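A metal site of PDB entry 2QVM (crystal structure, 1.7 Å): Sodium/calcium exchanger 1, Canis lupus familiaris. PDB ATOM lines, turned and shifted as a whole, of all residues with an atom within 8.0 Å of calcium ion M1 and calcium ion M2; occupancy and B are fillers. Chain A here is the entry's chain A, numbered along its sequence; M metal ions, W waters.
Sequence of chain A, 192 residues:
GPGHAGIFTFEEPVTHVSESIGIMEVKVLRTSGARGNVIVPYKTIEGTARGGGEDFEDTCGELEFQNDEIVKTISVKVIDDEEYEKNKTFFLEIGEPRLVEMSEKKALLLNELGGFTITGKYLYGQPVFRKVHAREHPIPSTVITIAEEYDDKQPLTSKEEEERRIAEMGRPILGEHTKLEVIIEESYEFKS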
ATOM      1  N   GLU A  19      -2.460 -22.168  -0.792  1.00  0.00           N
ATOM      2  CA  GLU A  19      -1.322 -22.855  -1.427  1.00  0.00           C
ATOM      3  C   GLU A  19      -0.456 -23.577  -0.362  1.00  0.00           C
ATOM      4  O   GLU A  19       0.280 -24.518  -0.700  1.00  0.00           O
ATOM      5  CB  GLU A  19      -0.479 -21.854  -2.226  1.00  0.00           C
ATOM      6  CG  GLU A  19       0.581 -22.451  -3.140  1.00  0.00           C
ATOM      7  CD  GLU A  19       1.448 -21.371  -3.818  1.00  0.00           C
ATOM      8  OE1 GLU A  19       1.247 -20.188  -3.523  1.00  0.00           O
ATOM      9  OE2 GLU A  19       2.301 -21.725  -4.623  1.00  0.00           O
ATOM     10  N   SER A  20      -0.593 -23.155   0.885  1.00  0.00           N
ATOM     11  CA  SER A  20       0.206 -23.721   1.989  1.00  0.00           C
ATOM     12  C   SER A  20      -0.577 -24.724   2.845  1.00  0.00           C
ATOM     13  O   SER A  20      -0.147 -25.102   3.931  1.00  0.00           O
ATOM     14  CB  SER A  20       0.785 -22.591   2.864  1.00  0.00           C
ATOM     15  OG  SER A  20      -0.247 -21.925   3.577  1.00  0.00           O
ATOM     16  N   THR A  48      -5.778 -24.689 -14.174  1.00  0.00           N
ATOM     17  CA  THR A  48      -4.542 -23.905 -14.351  1.00  0.00           C
ATOM     18  C   THR A  48      -3.445 -24.384 -13.381  1.00  0.00           C
ATOM     19  O   THR A  48      -2.253 -24.101 -13.573  1.00  0.00           O
ATOM     20  CB  THR A  48      -4.790 -22.418 -14.174  1.00  0.00           C
ATOM     21  OG1 THR A  48      -5.343 -22.164 -12.887  1.00  0.00           O
ATOM     22  CG2 THR A  48      -5.742 -21.898 -15.254  1.00  0.00           C
ATOM     23  N   ALA A  49      -3.847 -25.095 -12.326  1.00  0.00           N
ATOM     24  CA  ALA A  49      -2.902 -25.799 -11.481  1.00  0.00           C
ATOM     25  C   ALA A  49      -2.529 -27.114 -12.126  1.00  0.00           C
ATOM     26  O   ALA A  49      -3.399 -27.851 -12.617  1.00  0.00           O
ATOM     27  CB  ALA A  49      -3.475 -26.043 -10.062  1.00  0.00           C
ATOM     28  N   ARG A  50      -1.228 -27.414 -12.116  1.00  0.00           N
ATOM     29  CA  ARG A  50      -0.691 -28.612 -12.761  1.00  0.00           C
ATOM     30  C   ARG A  50      -0.587 -29.733 -11.772  1.00  0.00           C
ATOM     31  O   ARG A  50      -0.146 -29.552 -10.623  1.00  0.00           O
ATOM     32  CB  ARG A  50       0.706 -28.359 -13.353  1.00  0.00           C
ATOM     33  CG  ARG A  50       0.847 -27.051 -14.135  1.00  0.00           C
ATOM     34  CD  ARG A  50      -0.207 -26.878 -15.201  1.00  0.00           C
ATOM     35  NE  ARG A  50      -0.098 -27.881 -16.252  1.00  0.00           N
ATOM     36  CZ  ARG A  50      -0.934 -27.957 -17.287  1.00  0.00           C
ATOM     37  NH1 ARG A  50      -1.946 -27.101 -17.403  1.00  0.00           N
ATOM     38  NH2 ARG A  50      -0.761 -28.919 -18.200  1.00  0.00           N
ATOM     39  N   GLY A  53       2.344 -33.769  -9.375  1.00  0.00           N
ATOM     40  CA  GLY A  53       3.186 -33.368  -8.256  1.00  0.00           C
ATOM     41  C   GLY A  53       3.760 -31.965  -8.392  1.00  0.00           C
ATOM     42  O   GLY A  53       4.591 -31.569  -7.593  1.00  0.00           O
ATOM     43  N   GLU A  54       3.325 -31.228  -9.413  1.00  0.00           N
ATOM     44  CA  GLU A  54       3.786 -29.862  -9.598  1.00  0.00           C
ATOM     45  C   GLU A  54       3.095 -28.928  -8.590  1.00  0.00           C
ATOM     46  O   GLU A  54       3.724 -28.507  -7.633  1.00  0.00           O
ATOM     47  CB  GLU A  54       3.588 -29.412 -11.048  1.00  0.00           C
ATOM     48  CG  GLU A  54       4.201 -28.044 -11.355  1.00  0.00           C
ATOM     49  CD  GLU A  54       5.689 -27.998 -11.046  1.00  0.00           C
ATOM     50  OE1 GLU A  54       6.427 -28.900 -11.494  1.00  0.00           O
ATOM     51  OE2 GLU A  54       6.122 -27.057 -10.347  1.00  0.00           O
ATOM     52  N   ASP A  55       1.805 -28.645  -8.807  1.00  0.00           N
ATOM     53  CA  ASP A  55       0.973 -27.843  -7.879  1.00  0.00           C
ATOM     54  C   ASP A  55       0.138 -28.712  -6.964  1.00  0.00           C
ATOM     55  O   ASP A  55      -0.266 -28.293  -5.859  1.00  0.00           O
ATOM     56  CB  ASP A  55       0.039 -26.893  -8.650  1.00  0.00           C
ATOM     57  CG  ASP A  55       0.817 -25.903  -9.507  1.00  0.00           C
ATOM     58  OD1 ASP A  55       1.884 -25.444  -9.021  1.00  0.00           O
ATOM     59  OD2 ASP A  55       0.434 -25.673 -10.668  1.00  0.00           O
ATOM     60  N   PHE A  56      -0.145 -29.924  -7.440  1.00  0.00           N
ATOM     61  CA  PHE A  56      -0.834 -30.919  -6.605  1.00  0.00           C
ATOM     62  C   PHE A  56      -0.481 -32.320  -7.094  1.00  0.00           C
ATOM     63  O   PHE A  56      -0.011 -32.521  -8.231  1.00  0.00           O
ATOM     64  CB  PHE A  56      -2.369 -30.685  -6.620  1.00  0.00           C
ATOM     65  CG  PHE A  56      -3.019 -31.023  -7.939  1.00  0.00           C
ATOM     66  CD1 PHE A  56      -3.104 -30.076  -8.953  1.00  0.00           C
ATOM     67  CD2 PHE A  56      -3.519 -32.296  -8.170  1.00  0.00           C
ATOM     68  CE1 PHE A  56      -3.704 -30.397 -10.194  1.00  0.00           C
ATOM     69  CE2 PHE A  56      -4.111 -32.636  -9.398  1.00  0.00           C
ATOM     70  CZ  PHE A  56      -4.197 -31.682 -10.406  1.00  0.00           C
ATOM     71  N   ILE A  79       0.949 -28.644  -3.250  1.00  0.00           N
ATOM     72  CA  ILE A  79       2.389 -28.428  -3.184  1.00  0.00           C
ATOM     73  C   ILE A  79       2.688 -26.932  -3.174  1.00  0.00           C
ATOM     74  O   ILE A  79       2.376 -26.230  -4.144  1.00  0.00           O
ATOM     75  CB  ILE A  79       3.108 -29.111  -4.372  1.00  0.00           C
ATOM     76  CG1 ILE A  79       2.768 -30.627  -4.471  1.00  0.00           C
ATOM     77  CG2 ILE A  79       4.641 -28.795  -4.300  1.00  0.00           C
ATOM     78  CD1 ILE A  79       3.066 -31.404  -3.269  1.00  0.00           C
ATOM     79  N   ASP A  80       3.292 -26.449  -2.080  1.00  0.00           N
ATOM     80  CA  ASP A  80       3.589 -25.015  -1.925  1.00  0.00           C
ATOM     81  C   ASP A  80       4.854 -24.720  -2.742  1.00  0.00           C
ATOM     82  O   ASP A  80       5.602 -25.635  -3.096  1.00  0.00           O
ATOM     83  CB  ASP A  80       3.748 -24.687  -0.440  1.00  0.00           C
ATOM     84  CG  ASP A  80       3.508 -23.229  -0.129  1.00  0.00           C
ATOM     85  OD1 ASP A  80       3.271 -22.414  -1.067  1.00  0.00           O
ATOM     86  OD2 ASP A  80       3.558 -22.882   1.063  1.00  0.00           O
ATOM     87  N   ASP A  81       5.105 -23.457  -3.086  1.00  0.00           N
ATOM     88  CA  ASP A  81       6.326 -23.116  -3.785  1.00  0.00           C
ATOM     89  C   ASP A  81       6.862 -21.762  -3.321  1.00  0.00           C
ATOM     90  O   ASP A  81       6.349 -21.204  -2.359  1.00  0.00           O
ATOM     91  CB  ASP A  81       6.150 -23.146  -5.315  1.00  0.00           C
ATOM     92  CG  ASP A  81       5.169 -22.097  -5.831  1.00  0.00           C
ATOM     93  OD1 ASP A  81       5.008 -21.028  -5.179  1.00  0.00           O
ATOM     94  OD2 ASP A  81       4.601 -22.319  -6.919  1.00  0.00           O
ATOM     95  N   GLU A  82       7.888 -21.257  -4.008  1.00  0.00           N
ATOM     96  CA  GLU A  82       8.500 -19.978  -3.648  1.00  0.00           C
ATOM     97  C   GLU A  82       8.276 -18.891  -4.691  1.00  0.00           C
ATOM     98  O   GLU A  82       9.000 -17.872  -4.690  1.00  0.00           O
ATOM     99  CB  GLU A  82      10.001 -20.150  -3.393  1.00  0.00           C
ATOM    100  CG  GLU A  82      10.316 -21.002  -2.183  1.00  0.00           C
ATOM    101  CD  GLU A  82      11.797 -21.157  -1.976  1.00  0.00           C
ATOM    102  OE1 GLU A  82      12.441 -20.126  -1.691  1.00  0.00           O
ATOM    103  OE2 GLU A  82      12.321 -22.283  -2.102  1.00  0.00           O
ATOM    104  N   GLU A  83       7.293 -19.079  -5.569  1.00  0.00           N
ATOM    105  CA  GLU A  83       6.977 -18.145  -6.629  1.00  0.00           C
ATOM    106  C   GLU A  83       5.714 -17.371  -6.300  1.00  0.00           C
ATOM    107  O   GLU A  83       4.827 -17.894  -5.620  1.00  0.00           O
ATOM    108  CB  GLU A  83       6.756 -18.886  -7.957  1.00  0.00           C
ATOM    109  CG  GLU A  83       7.890 -19.865  -8.380  1.00  0.00           C
ATOM    110  CD  GLU A  83       9.267 -19.209  -8.492  1.00  0.00           C
ATOM    111  OE1 GLU A  83       9.358 -18.031  -8.934  1.00  0.00           O
ATOM    112  OE2 GLU A  83      10.278 -19.870  -8.141  1.00  0.00           O
ATOM    113  N   TYR A  84       5.630 -16.145  -6.791  1.00  0.00           N
ATOM    114  CA  TYR A  84       4.446 -15.323  -6.653  1.00  0.00           C
ATOM    115  C   TYR A  84       3.642 -15.377  -7.964  1.00  0.00           C
ATOM    116  O   TYR A  84       4.076 -14.855  -9.003  1.00  0.00           O
ATOM    117  CB  TYR A  84       4.821 -13.855  -6.348  1.00  0.00           C
ATOM    118  CG  TYR A  84       5.442 -13.537  -4.990  1.00  0.00           C
ATOM    119  CD1 TYR A  84       5.650 -14.525  -4.007  1.00  0.00           C
ATOM    120  CD2 TYR A  84       5.795 -12.228  -4.673  1.00  0.00           C
ATOM    121  CE1 TYR A  84       6.221 -14.199  -2.763  1.00  0.00           C
ATOM    122  CE2 TYR A  84       6.342 -11.893  -3.414  1.00  0.00           C
ATOM    123  CZ  TYR A  84       6.564 -12.909  -2.475  1.00  0.00           C
ATOM    124  OH  TYR A  84       7.125 -12.610  -1.232  1.00  0.00           O
ATOM    125  N   GLU A  85       2.467 -16.007  -7.924  1.00  0.00           N
ATOM    126  CA  GLU A  85       1.645 -16.193  -9.136  1.00  0.00           C
ATOM    127  C   GLU A  85       0.185 -15.942  -8.851  1.00  0.00           C
ATOM    128  O   GLU A  85      -0.211 -15.711  -7.702  1.00  0.00           O
ATOM    129  CB  GLU A  85       1.883 -17.600  -9.720  1.00  0.00           C
ATOM    130  CG  GLU A  85       3.351 -17.839 -10.041  1.00  0.00           C
ATOM    131  CD  GLU A  85       3.706 -19.274 -10.407  1.00  0.00           C
ATOM    132  OE1 GLU A  85       3.030 -20.206  -9.966  1.00  0.00           O
ATOM    133  OE2 GLU A  85       4.709 -19.462 -11.128  1.00  0.00           O
ATOM    134  N   LYS A  86      -0.638 -15.947  -9.898  1.00  0.00           N
ATOM    135  CA  LYS A  86      -2.076 -15.856  -9.695  1.00  0.00           C
ATOM    136  C   LYS A  86      -2.626 -17.132  -9.055  1.00  0.00           C
ATOM    137  O   LYS A  86      -1.934 -18.154  -9.036  1.00  0.00           O
ATOM    138  CB  LYS A  86      -2.768 -15.627 -11.030  1.00  0.00           C
ATOM    139  CG  LYS A  86      -2.431 -14.279 -11.635  1.00  0.00           C
ATOM    140  CD  LYS A  86      -2.413 -14.365 -13.156  1.00  0.00           C
ATOM    141  CE  LYS A  86      -1.959 -13.043 -13.746  1.00  0.00           C
ATOM    142  NZ  LYS A  86      -2.987 -11.974 -13.478  1.00  0.00           N
ATOM    143  N   LYS A  88      -4.694 -20.504  -8.730  1.00  0.00           N
ATOM    144  CA  LYS A  88      -4.760 -21.551  -9.747  1.00  0.00           C
ATOM    145  C   LYS A  88      -5.884 -22.489  -9.421  1.00  0.00           C
ATOM    146  O   LYS A  88      -6.298 -22.548  -8.264  1.00  0.00           O
ATOM    147  CB  LYS A  88      -3.438 -22.269  -9.817  1.00  0.00           C
ATOM    148  CG  LYS A  88      -2.367 -21.363 -10.506  1.00  0.00           C
ATOM    149  CD  LYS A  88      -1.087 -22.095 -10.567  1.00  0.00           C
ATOM    150  CE  LYS A  88       0.036 -21.127 -10.830  1.00  0.00           C
ATOM    151  NZ  LYS A  88       1.285 -21.924 -10.824  1.00  0.00           N
ATOM    152  N   ILE A 184      -6.769 -22.712  -5.571  1.00  0.00           N
ATOM    153  CA  ILE A 184      -5.592 -22.641  -4.683  1.00  0.00           C
ATOM    154  C   ILE A 184      -5.122 -21.178  -4.596  1.00  0.00           C
ATOM    155  O   ILE A 184      -4.643 -20.583  -5.604  1.00  0.00           O
ATOM    156  CB  ILE A 184      -4.428 -23.548  -5.169  1.00  0.00           C
ATOM    157  CG1 ILE A 184      -4.896 -24.985  -5.528  1.00  0.00           C
ATOM    158  CG2 ILE A 184      -3.292 -23.578  -4.109  1.00  0.00           C
ATOM    159  CD1 ILE A 184      -3.810 -25.856  -6.176  1.00  0.00           C
ATOM    160  N   GLU A 185      -5.275 -20.595  -3.428  1.00  0.00           N
ATOM    161  CA  GLU A 185      -4.913 -19.189  -3.215  1.00  0.00           C
ATOM    162  C   GLU A 185      -3.418 -19.022  -2.936  1.00  0.00           C
ATOM    163  O   GLU A 185      -2.884 -19.570  -1.968  1.00  0.00           O
ATOM    164  CB  GLU A 185      -5.722 -18.622  -2.062  1.00  0.00           C
ATOM    165  CG  GLU A 185      -7.245 -18.600  -2.409  1.00  0.00           C
ATOM    166  CD  GLU A 185      -8.159 -18.212  -1.239  1.00  0.00           C
ATOM    167  OE1 GLU A 185      -7.832 -18.520  -0.052  1.00  0.00           O
ATOM    168  OE2 GLU A 185      -9.217 -17.602  -1.529  1.00  0.00           O
ATOM    169  N   GLU A 186      -2.775 -18.207  -3.772  1.00  0.00           N
ATOM    170  CA  GLU A 186      -1.338 -17.900  -3.644  1.00  0.00           C
ATOM    171  C   GLU A 186      -0.979 -17.553  -2.185  1.00  0.00           C
ATOM    172  O   GLU A 186      -1.681 -16.761  -1.547  1.00  0.00           O
ATOM    173  CB  GLU A 186      -1.029 -16.733  -4.602  1.00  0.00           C
ATOM    174  CG  GLU A 186       0.363 -16.142  -4.399  1.00  0.00           C
ATOM    175  CD  GLU A 186       1.459 -17.139  -4.663  1.00  0.00           C
ATOM    176  OE1 GLU A 186       1.508 -17.788  -5.745  1.00  0.00           O
ATOM    177  OE2 GLU A 186       2.334 -17.274  -3.755  1.00  0.00           O
ATOM    178  N   SER A 187       0.068 -18.164  -1.646  1.00  0.00           N
ATOM    179  CA  SER A 187       0.433 -17.987  -0.242  1.00  0.00           C
ATOM    180  C   SER A 187       1.508 -16.923  -0.029  1.00  0.00           C
ATOM    181  O   SER A 187       1.704 -16.459   1.086  1.00  0.00           O
ATOM    182  CB  SER A 187       0.932 -19.314   0.350  1.00  0.00           C
ATOM    183  OG  SER A 187       2.102 -19.747  -0.343  1.00  0.00           O
ATOM    184  N   TYR A 188       2.194 -16.541  -1.117  1.00  0.00           N
ATOM    185  CA  TYR A 188       3.340 -15.603  -1.059  1.00  0.00           C
ATOM    186  C   TYR A 188       4.424 -16.054  -0.062  1.00  0.00           C
ATOM    187  O   TYR A 188       4.666 -17.254   0.093  1.00  0.00           O
ATOM    188  CB  TYR A 188       2.899 -14.153  -0.809  1.00  0.00           C
ATOM    189  CG  TYR A 188       1.916 -13.652  -1.817  1.00  0.00           C
ATOM    190  CD1 TYR A 188       2.330 -13.187  -3.065  1.00  0.00           C
ATOM    191  CD2 TYR A 188       0.557 -13.617  -1.509  1.00  0.00           C
ATOM    192  CE1 TYR A 188       1.403 -12.717  -3.992  1.00  0.00           C
ATOM    193  CE2 TYR A 188      -0.383 -13.157  -2.443  1.00  0.00           C
ATOM    194  CZ  TYR A 188       0.060 -12.704  -3.666  1.00  0.00           C
ATOM    195  OH  TYR A 188      -0.875 -12.239  -4.571  1.00  0.00           O
HETATM  196 CA    CA M   1       3.220 -19.475  -4.917  1.00  0.00          CA
HETATM  197 CA    CA M   2       3.382 -24.035  -7.923  1.00  0.00          CA
HETATM  198  O   HOH W   1       1.407 -22.475  -8.063  1.00  0.00           O
HETATM  199  O   HOH W   2       2.334 -24.086  -5.662  1.00  0.00           O
HETATM  200  O   HOH W   3       2.979 -20.097  -7.267  1.00  0.00           O
HETATM  201  O   HOH W   4       5.240 -24.773  -9.197  1.00  0.00           O
HETATM  202  O   HOH W   5       4.137 -25.944  -6.713  1.00  0.00           O
HETATM  203  O   HOH W   6       3.747 -22.838 -10.076  1.00  0.00           O
HETATM  204  O   HOH W   7       4.230 -19.468  -2.727  1.00  0.00           O
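The side-chain carboxylate (OE1) of Glu 186 sits close to the backbone NH (N) of Glu 85. The backbone carbonyl oxygen of Asp 55 sits at hydrogen-bond distance from the backbone NH of Ile 79 (2.9 Å). N of Glu 19 lies within hydrogen-bond range of O of Glu 185, 2.9 Å away. N of Ser 187 sits close to OE1 of Glu 19, at 3.0 Å. OD2 of Asp 55 lies within salt-bridge range of NZ of Lys 88 (3.8 Å). The side-chain carboxylate of Glu 186 sits close to the backbone NH of Tyr 188 (2.7 Å). The side-chain carboxylate of Asp 55 is in hydrogen-bond range of the backbone NH of Arg 50 (2.8 Å).
The nearest printed residue that does not touch calcium ion M1 is Tyr 84 (4.5 Å).
Two residues have an atom within 4 Å of calcium ion M2: Asp 55 and Asp 81. The nearest printed residue that does not touch calcium ion M2 is Lys 88 (4.2 Å).
O of Glu 83 is bound to calcium ion M1 (2.4 Å). The side-chain carboxylate (OD1) of Asp 81 is bound to calcium ion M1, 2.4 Å away. Water W7 binds calcium ion M1. Calcium ion M1 is bound by water W3, at 2.4 Å. OE2 of Glu 19 is bound to calcium ion M1 (2.4 Å). Calcium ion M1 is bound by OE1 of Glu 19 (2.5 Å). The side-chain carboxylate (OE1) of Glu 186 binds calcium ion M1 (2.5 Å). The side-chain carboxylate (OE2) of Glu 186 is bound to calcium ion M1 (2.6 Å).
Calcium ion M2 is bound by OD2 of Asp 81 (2.3 Å). OD1 of Asp 55 is bound to calcium ion M2. Water W4 binds calcium ion M2 (2.4 Å). Calcium ion M2 is bound by water W5, 2.4 Å away. Water W6 is bound to calcium ion M2 (2.5 Å). Water W2 is bound to calcium ion M2 (2.5 Å). Water W1 binds calcium ion M2 (2.5 Å). Calcium ion M2 has seven donor atoms within binding distance.
Water W7 bridges the backbone carbonyl oxygen (O) of Asp 81 and the side-chain hydroxyl (OG) of Ser 187. Water W5 bridges O of Glu 54 (2.8 Å) and O of Ile 79 (3.1 Å). Water W6 lies within hydrogen-bond range of OE1 of Glu 85 and NZ of Lys 88. Water W1 bridges the side-chain amino group of Lys 88 (2.8 Å) and the side-chain carboxylate of Glu 85 (3.4 Å).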
